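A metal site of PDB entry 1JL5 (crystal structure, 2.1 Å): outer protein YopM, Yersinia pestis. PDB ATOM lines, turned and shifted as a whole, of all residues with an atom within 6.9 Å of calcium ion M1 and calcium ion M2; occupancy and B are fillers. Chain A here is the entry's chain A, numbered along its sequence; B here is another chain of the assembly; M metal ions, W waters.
The backbone carbonyl oxygen (O) of Asp 266 sits at hydrogen-bond distance from the side-chain amino group (NZ) of Lys 328 of chain B (2.6 Å). The backbone carbonyl oxygen of Asp 266 is in hydrogen-bond range of the backbone NH of Asn 247 (3.4 Å). O of Arg 265 sits at hydrogen-bond distance from N of Asn 246 (2.5 Å). N of Asn 307 of chain B is in hydrogen-bond range of OD1 of Asn 327 of chain B, 2.9 Å away. The side-chain amide oxygen (OD1) of Asn 307 of chain B lies close to the backbone NH (N) of Asn 287 of chain B, at 2.9 Å. The side-chain amide oxygen (OD1) of Asn 307 of chain B lies close to the backbone NH (N) of Phe 289 of chain B (3.1 Å). The backbone NH (N) of Glu 308 of chain B sits at hydrogen-bond distance from the side-chain amide oxygen (OD1) of Asn 327 of chain B. N of Asn 267 sits at hydrogen-bond distance from O of Glu 286 (3.1 Å).
Three residues have an atom within 4 Å of calcium ion M1: Asp 266, Asn 307 of chain B and Glu 308 of chain B. The nearest printed residue that does not touch calcium ion M1 is Lys 328 of chain B (4.04 Å).
Calcium ion M1 is bound by the side-chain carboxylate of Asp 266 (2.2 Å), the backbone carbonyl oxygen of Asn 307 of chain B (2.3 Å), the side-chain carboxylate of Glu 308 of chain B (2.3 Å), water W4 (2.3 Å), water W3 (2.4 Å), water W2 (2.5 Å) and water W1 (2.8 Å). Calcium ion M1 has seven donor atoms within binding distance.
The side-chain carboxylate (OD2) of Asp 266 binds calcium ion M2, at 2.0 Å. Calcium ion M2 is bound by OD1 of Asn 246 (2.0 Å). Water W7 binds calcium ion M2 (2.2 Å). Water W6 is bound to calcium ion M2. The side-chain amide oxygen (OD1) of Asn 326 of chain B is bound to calcium ion M2, at 2.2 Å. Calcium ion M2 is bound by water W5 (2.3 Å). Calcium ion M2 has six donor atoms within binding distance.
Glu 286 touches calcium ion M2 (OE1 to CA, 3.9 Å). Of the 22 residues printed, 4 come within 4 Å of calcium ion M2. The nearest printed residue that does not touch calcium ion M2 is Lys 328 of chain B (4.5 Å).
Water W1 bridges the backbone carbonyl oxygen of Ser 306 of chain B (3.2 Å) and the backbone carbonyl oxygen of Asn 287 of chain B (3.3 Å). Water W4 lies within hydrogen-bond range of the side-chain carboxylate of Glu 286 (2.7 Å) and the side-chain amide nitrogen of Asn 326 of chain B (3.5 Å). Water W2 lies within hydrogen-bond range of the backbone carbonyl oxygen (O) of Asn 267 (2.4 Å) and the backbone carbonyl oxygen (O) of Glu 286 (2.7 Å). Water W5 lies within hydrogen-bond range of O of Asn 327 of chain B and O of Phe 346 of chain B.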
ATOM      1  N   ASN A 224     -13.155 -28.577  10.417  1.00  0.00           N
ATOM      2  CA  ASN A 224     -12.787 -27.937  11.653  1.00  0.00           C
ATOM      3  C   ASN A 224     -12.638 -28.849  12.833  1.00  0.00           C
ATOM      4  O   ASN A 224     -13.131 -28.581  13.924  1.00  0.00           O
ATOM      5  CB  ASN A 224     -13.769 -26.844  11.992  1.00  0.00           C
ATOM      6  CG  ASN A 224     -13.313 -25.525  11.473  1.00  0.00           C
ATOM      7  OD1 ASN A 224     -12.237 -25.058  11.838  1.00  0.00           O
ATOM      8  ND2 ASN A 224     -14.104 -24.917  10.602  1.00  0.00           N
ATOM      9  N   ASP A 245     -12.904 -30.018   5.673  1.00  0.00           N
ATOM     10  CA  ASP A 245     -12.209 -28.760   5.604  1.00  0.00           C
ATOM     11  C   ASP A 245     -11.646 -28.469   6.973  1.00  0.00           C
ATOM     12  O   ASP A 245     -12.064 -29.063   7.964  1.00  0.00           O
ATOM     13  CB  ASP A 245     -13.177 -27.645   5.239  1.00  0.00           C
ATOM     14  CG  ASP A 245     -14.342 -27.567   6.207  1.00  0.00           C
ATOM     15  OD1 ASP A 245     -15.210 -28.472   6.162  1.00  0.00           O
ATOM     16  OD2 ASP A 245     -14.389 -26.637   7.028  1.00  0.00           O
ATOM     17  N   ASN A 246     -10.678 -27.570   7.026  1.00  0.00           N
ATOM     18  CA  ASN A 246     -10.117 -27.154   8.289  1.00  0.00           C
ATOM     19  C   ASN A 246      -9.718 -28.271   9.210  1.00  0.00           C
ATOM     20  O   ASN A 246     -10.099 -28.297  10.374  1.00  0.00           O
ATOM     21  CB  ASN A 246     -11.100 -26.230   8.978  1.00  0.00           C
ATOM     22  CG  ASN A 246     -11.242 -24.935   8.244  1.00  0.00           C
ATOM     23  OD1 ASN A 246     -10.298 -24.150   8.199  1.00  0.00           O
ATOM     24  ND2 ASN A 246     -12.400 -24.709   7.638  1.00  0.00           N
ATOM     25  N   ASN A 247      -8.946 -29.195   8.667  1.00  0.00           N
ATOM     26  CA  ASN A 247      -8.455 -30.288   9.465  1.00  0.00           C
ATOM     27  C   ASN A 247      -6.966 -30.310   9.287  1.00  0.00           C
ATOM     28  O   ASN A 247      -6.372 -29.291   8.945  1.00  0.00           O
ATOM     29  CB  ASN A 247      -9.115 -31.593   9.026  1.00  0.00           C
ATOM     30  CG  ASN A 247     -10.461 -31.779   9.671  1.00  0.00           C
ATOM     31  OD1 ASN A 247     -10.560 -31.897  10.889  1.00  0.00           O
ATOM     32  ND2 ASN A 247     -11.516 -31.809   8.865  1.00  0.00           N
ATOM     33  N   ARG A 265     -11.385 -27.856   2.227  1.00  0.00           N
ATOM     34  CA  ARG A 265     -10.853 -26.513   2.306  1.00  0.00           C
ATOM     35  C   ARG A 265      -9.971 -26.424   3.527  1.00  0.00           C
ATOM     36  O   ARG A 265     -10.277 -26.967   4.583  1.00  0.00           O
ATOM     37  CB  ARG A 265     -11.995 -25.501   2.415  1.00  0.00           C
ATOM     38  CG  ARG A 265     -11.552 -24.101   2.805  1.00  0.00           C
ATOM     39  CD  ARG A 265     -12.764 -23.198   2.848  1.00  0.00           C
ATOM     40  NE  ARG A 265     -12.506 -21.895   3.456  1.00  0.00           N
ATOM     41  CZ  ARG A 265     -11.846 -20.899   2.873  1.00  0.00           C
ATOM     42  NH1 ARG A 265     -11.364 -21.042   1.640  1.00  0.00           N
ATOM     43  NH2 ARG A 265     -11.676 -19.754   3.524  1.00  0.00           N
ATOM     44  N   ASP A 266      -8.867 -25.732   3.356  1.00  0.00           N
ATOM     45  CA  ASP A 266      -7.925 -25.521   4.424  1.00  0.00           C
ATOM     46  C   ASP A 266      -7.444 -26.802   5.058  1.00  0.00           C
ATOM     47  O   ASP A 266      -7.844 -27.192   6.158  1.00  0.00           O
ATOM     48  CB  ASP A 266      -8.507 -24.619   5.490  1.00  0.00           C
ATOM     49  CG  ASP A 266      -7.437 -24.088   6.414  1.00  0.00           C
ATOM     50  OD1 ASP A 266      -6.286 -24.551   6.278  1.00  0.00           O
ATOM     51  OD2 ASP A 266      -7.738 -23.215   7.241  1.00  0.00           O
ATOM     52  N   ASN A 267      -6.561 -27.469   4.333  1.00  0.00           N
ATOM     53  CA  ASN A 267      -5.938 -28.675   4.804  1.00  0.00           C
ATOM     54  C   ASN A 267      -4.563 -28.567   4.220  1.00  0.00           C
ATOM     55  O   ASN A 267      -4.177 -27.501   3.752  1.00  0.00           O
ATOM     56  CB  ASN A 267      -6.679 -29.909   4.322  1.00  0.00           C
ATOM     57  CG  ASN A 267      -7.825 -30.259   5.243  1.00  0.00           C
ATOM     58  OD1 ASN A 267      -7.610 -30.664   6.388  1.00  0.00           O
ATOM     59  ND2 ASN A 267      -9.057 -30.097   4.769  1.00  0.00           N
ATOM     60  N   TYR A 268      -3.810 -29.642   4.223  1.00  0.00           N
ATOM     61  CA  TYR A 268      -2.465 -29.550   3.723  1.00  0.00           C
ATOM     62  C   TYR A 268      -2.333 -30.401   2.494  1.00  0.00           C
ATOM     63  O   TYR A 268      -1.328 -31.089   2.317  1.00  0.00           O
ATOM     64  CB  TYR A 268      -1.499 -30.016   4.795  1.00  0.00           C
ATOM     65  CG  TYR A 268      -0.153 -29.374   4.697  1.00  0.00           C
ATOM     66  CD1 TYR A 268      -0.004 -28.008   4.905  1.00  0.00           C
ATOM     67  CD2 TYR A 268       0.980 -30.133   4.419  1.00  0.00           C
ATOM     68  CE1 TYR A 268       1.244 -27.408   4.850  1.00  0.00           C
ATOM     69  CE2 TYR A 268       2.229 -29.544   4.356  1.00  0.00           C
ATOM     70  CZ  TYR A 268       2.356 -28.186   4.571  1.00  0.00           C
ATOM     71  OH  TYR A 268       3.590 -27.612   4.514  1.00  0.00           O
ATOM     72  N   GLU A 286      -7.489 -23.206   0.069  1.00  0.00           N
ATOM     73  CA  GLU A 286      -6.618 -23.185   1.225  1.00  0.00           C
ATOM     74  C   GLU A 286      -5.913 -24.489   1.509  1.00  0.00           C
ATOM     75  O   GLU A 286      -5.882 -24.963   2.627  1.00  0.00           O
ATOM     76  CB  GLU A 286      -7.380 -22.768   2.470  1.00  0.00           C
ATOM     77  CG  GLU A 286      -7.613 -21.281   2.548  1.00  0.00           C
ATOM     78  CD  GLU A 286      -8.235 -20.896   3.853  1.00  0.00           C
ATOM     79  OE1 GLU A 286      -7.639 -21.167   4.909  1.00  0.00           O
ATOM     80  OE2 GLU A 286      -9.330 -20.327   3.834  1.00  0.00           O
ATOM     81  N   ASN A 287      -5.383 -25.084   0.455  1.00  0.00           N
ATOM     82  CA  ASN A 287      -4.605 -26.262   0.643  1.00  0.00           C
ATOM     83  C   ASN A 287      -3.286 -25.851   0.063  1.00  0.00           C
ATOM     84  O   ASN A 287      -3.001 -24.659   0.000  1.00  0.00           O
ATOM     85  CB  ASN A 287      -5.239 -27.441  -0.074  1.00  0.00           C
ATOM     86  CG  ASN A 287      -6.242 -28.133   0.813  1.00  0.00           C
ATOM     87  OD1 ASN A 287      -5.869 -28.931   1.653  1.00  0.00           O
ATOM     88  ND2 ASN A 287      -7.514 -27.800   0.647  1.00  0.00           N
ATOM     89  N   ILE A 288      -2.472 -26.797  -0.364  1.00  0.00           N
ATOM     90  CA  ILE A 288      -1.199 -26.383  -0.885  1.00  0.00           C
ATOM     91  C   ILE A 288      -0.984 -26.926  -2.274  1.00  0.00           C
ATOM     92  O   ILE A 288       0.085 -27.401  -2.628  1.00  0.00           O
ATOM     93  CB  ILE A 288      -0.075 -26.794   0.064  1.00  0.00           C
ATOM     94  CG1 ILE A 288      -0.039 -28.314   0.248  1.00  0.00           C
ATOM     95  CG2 ILE A 288      -0.321 -26.152   1.423  1.00  0.00           C
ATOM     96  CD1 ILE A 288       1.130 -28.779   1.110  1.00  0.00           C
ATOM     97  N   ASN B 287       1.415 -19.347   3.701  1.00  0.00           N
ATOM     98  CA  ASN B 287       2.469 -20.151   3.179  1.00  0.00           C
ATOM     99  C   ASN B 287       2.039 -21.524   3.598  1.00  0.00           C
ATOM    100  O   ASN B 287       0.852 -21.740   3.824  1.00  0.00           O
ATOM    101  CB  ASN B 287       3.803 -19.730   3.768  1.00  0.00           C
ATOM    102  CG  ASN B 287       4.429 -18.630   2.950  1.00  0.00           C
ATOM    103  OD1 ASN B 287       5.034 -18.899   1.924  1.00  0.00           O
ATOM    104  ND2 ASN B 287       4.247 -17.389   3.381  1.00  0.00           N
ATOM    105  N   PHE B 289       3.393 -23.368   6.258  1.00  0.00           N
ATOM    106  CA  PHE B 289       4.055 -23.691   7.497  1.00  0.00           C
ATOM    107  C   PHE B 289       3.114 -24.561   8.310  1.00  0.00           C
ATOM    108  O   PHE B 289       1.934 -24.235   8.459  1.00  0.00           O
ATOM    109  CB  PHE B 289       4.359 -22.417   8.278  1.00  0.00           C
ATOM    110  CG  PHE B 289       5.456 -21.616   7.671  1.00  0.00           C
ATOM    111  CD1 PHE B 289       6.779 -21.957   7.912  1.00  0.00           C
ATOM    112  CD2 PHE B 289       5.176 -20.542   6.845  1.00  0.00           C
ATOM    113  CE1 PHE B 289       7.813 -21.244   7.318  1.00  0.00           C
ATOM    114  CE2 PHE B 289       6.198 -19.827   6.245  1.00  0.00           C
ATOM    115  CZ  PHE B 289       7.528 -20.175   6.485  1.00  0.00           C
ATOM    116  N   SER B 306      -3.203 -18.108   8.079  1.00  0.00           N
ATOM    117  CA  SER B 306      -3.466 -18.906   6.890  1.00  0.00           C
ATOM    118  C   SER B 306      -2.319 -19.785   6.433  1.00  0.00           C
ATOM    119  O   SER B 306      -1.969 -19.828   5.262  1.00  0.00           O
ATOM    120  CB  SER B 306      -3.927 -18.003   5.760  1.00  0.00           C
ATOM    121  OG  SER B 306      -5.200 -17.483   6.109  1.00  0.00           O
ATOM    122  N   ASN B 307      -1.714 -20.458   7.397  1.00  0.00           N
ATOM    123  CA  ASN B 307      -0.662 -21.401   7.116  1.00  0.00           C
ATOM    124  C   ASN B 307      -1.333 -22.651   7.597  1.00  0.00           C
ATOM    125  O   ASN B 307      -2.552 -22.733   7.585  1.00  0.00           O
ATOM    126  CB  ASN B 307       0.587 -21.069   7.927  1.00  0.00           C
ATOM    127  CG  ASN B 307       1.499 -20.131   7.196  1.00  0.00           C
ATOM    128  OD1 ASN B 307       2.146 -20.523   6.231  1.00  0.00           O
ATOM    129  ND2 ASN B 307       1.535 -18.866   7.625  1.00  0.00           N
ATOM    130  N   GLU B 308      -0.561 -23.628   8.025  1.00  0.00           N
ATOM    131  CA  GLU B 308      -1.160 -24.831   8.537  1.00  0.00           C
ATOM    132  C   GLU B 308      -0.489 -25.014   9.886  1.00  0.00           C
ATOM    133  O   GLU B 308      -0.185 -26.119  10.300  1.00  0.00           O
ATOM    134  CB  GLU B 308      -0.882 -26.008   7.603  1.00  0.00           C
ATOM    135  CG  GLU B 308      -1.778 -27.187   7.890  1.00  0.00           C
ATOM    136  CD  GLU B 308      -3.217 -26.930   7.510  1.00  0.00           C
ATOM    137  OE1 GLU B 308      -3.605 -25.742   7.374  1.00  0.00           O
ATOM    138  OE2 GLU B 308      -3.958 -27.903   7.351  1.00  0.00           O
ATOM    139  N   ILE B 309      -0.247 -23.885  10.545  1.00  0.00           N
ATOM    140  CA  ILE B 309       0.423 -23.894  11.829  1.00  0.00           C
ATOM    141  C   ILE B 309      -0.353 -24.687  12.857  1.00  0.00           C
ATOM    142  O   ILE B 309      -1.465 -24.324  13.235  1.00  0.00           O
ATOM    143  CB  ILE B 309       0.599 -22.467  12.393  1.00  0.00           C
ATOM    144  CG1 ILE B 309       1.359 -21.594  11.376  1.00  0.00           C
ATOM    145  CG2 ILE B 309       1.330 -22.535  13.717  1.00  0.00           C
ATOM    146  CD1 ILE B 309       2.676 -22.150  10.985  1.00  0.00           C
ATOM    147  N   ASN B 326      -6.430 -18.213  11.204  1.00  0.00           N
ATOM    148  CA  ASN B 326      -6.617 -19.234  10.212  1.00  0.00           C
ATOM    149  C   ASN B 326      -5.457 -20.203  10.107  1.00  0.00           C
ATOM    150  O   ASN B 326      -4.791 -20.307   9.084  1.00  0.00           O
ATOM    151  CB  ASN B 326      -6.870 -18.595   8.848  1.00  0.00           C
ATOM    152  CG  ASN B 326      -7.281 -19.610   7.818  1.00  0.00           C
ATOM    153  OD1 ASN B 326      -7.925 -20.606   8.158  1.00  0.00           O
ATOM    154  ND2 ASN B 326      -6.929 -19.377   6.566  1.00  0.00           N
ATOM    155  N   ASN B 327      -5.222 -20.909  11.194  1.00  0.00           N
ATOM    156  CA  ASN B 327      -4.187 -21.916  11.205  1.00  0.00           C
ATOM    157  C   ASN B 327      -4.824 -23.117  11.826  1.00  0.00           C
ATOM    158  O   ASN B 327      -6.038 -23.236  11.816  1.00  0.00           O
ATOM    159  CB  ASN B 327      -2.970 -21.431  11.986  1.00  0.00           C
ATOM    160  CG  ASN B 327      -2.018 -20.662  11.097  1.00  0.00           C
ATOM    161  OD1 ASN B 327      -1.446 -21.227  10.172  1.00  0.00           O
ATOM    162  ND2 ASN B 327      -1.863 -19.370  11.367  1.00  0.00           N
ATOM    163  N   LYS B 328      -4.028 -24.022  12.360  1.00  0.00           N
ATOM    164  CA  LYS B 328      -4.591 -25.218  12.950  1.00  0.00           C
ATOM    165  C   LYS B 328      -4.112 -25.343  14.373  1.00  0.00           C
ATOM    166  O   LYS B 328      -3.853 -26.435  14.869  1.00  0.00           O
ATOM    167  CB  LYS B 328      -4.188 -26.434  12.119  1.00  0.00           C
ATOM    168  CG  LYS B 328      -4.672 -26.324  10.681  1.00  0.00           C
ATOM    169  CD  LYS B 328      -6.191 -26.305  10.624  1.00  0.00           C
ATOM    170  CE  LYS B 328      -6.692 -25.918   9.242  1.00  0.00           C
ATOM    171  NZ  LYS B 328      -6.171 -26.805   8.159  1.00  0.00           N
ATOM    172  N   PHE B 346      -9.992 -18.152  13.703  1.00  0.00           N
ATOM    173  CA  PHE B 346      -9.980 -19.258  12.755  1.00  0.00           C
ATOM    174  C   PHE B 346      -8.883 -20.257  13.056  1.00  0.00           C
ATOM    175  O   PHE B 346      -8.049 -20.579  12.212  1.00  0.00           O
ATOM    176  CB  PHE B 346      -9.834 -18.706  11.338  1.00  0.00           C
ATOM    177  CG  PHE B 346     -10.968 -17.846  10.922  1.00  0.00           C
ATOM    178  CD1 PHE B 346     -12.214 -18.418  10.659  1.00  0.00           C
ATOM    179  CD2 PHE B 346     -10.814 -16.475  10.795  1.00  0.00           C
ATOM    180  CE1 PHE B 346     -13.286 -17.629  10.274  1.00  0.00           C
ATOM    181  CE2 PHE B 346     -11.881 -15.681  10.404  1.00  0.00           C
ATOM    182  CZ  PHE B 346     -13.121 -16.248  10.148  1.00  0.00           C
ATOM    183  N   ASN B 347      -8.902 -20.726  14.277  1.00  0.00           N
ATOM    184  CA  ASN B 347      -7.951 -21.731  14.706  1.00  0.00           C
ATOM    185  C   ASN B 347      -8.763 -22.711  15.505  1.00  0.00           C
ATOM    186  O   ASN B 347      -9.979 -22.620  15.535  1.00  0.00           O
ATOM    187  CB  ASN B 347      -6.857 -21.095  15.555  1.00  0.00           C
ATOM    188  CG  ASN B 347      -5.724 -20.580  14.718  1.00  0.00           C
ATOM    189  OD1 ASN B 347      -4.966 -21.362  14.150  1.00  0.00           O
ATOM    190  ND2 ASN B 347      -5.625 -19.275  14.600  1.00  0.00           N
HETATM  191 CA    CA M   1      -4.201 -23.756   6.397  1.00  0.00          CA
HETATM  192 CA    CA M   2      -9.272 -22.393   8.281  1.00  0.00          CA
HETATM  193  O   HOH W   1      -2.138 -22.931   4.673  1.00  0.00           O
HETATM  194  O   HOH W   2      -3.830 -25.174   4.387  1.00  0.00           O
HETATM  195  O   HOH W   3      -5.351 -22.883   8.265  1.00  0.00           O
HETATM  196  O   HOH W   4      -5.135 -22.007   5.229  1.00  0.00           O
HETATM  197  O   HOH W   5      -8.104 -22.823  10.245  1.00  0.00           O
HETATM  198  O   HOH W   6     -11.037 -21.393   9.198  1.00  0.00           O
HETATM  199  O   HOH W   7      -9.904 -21.604   6.319  1.00  0.00           O
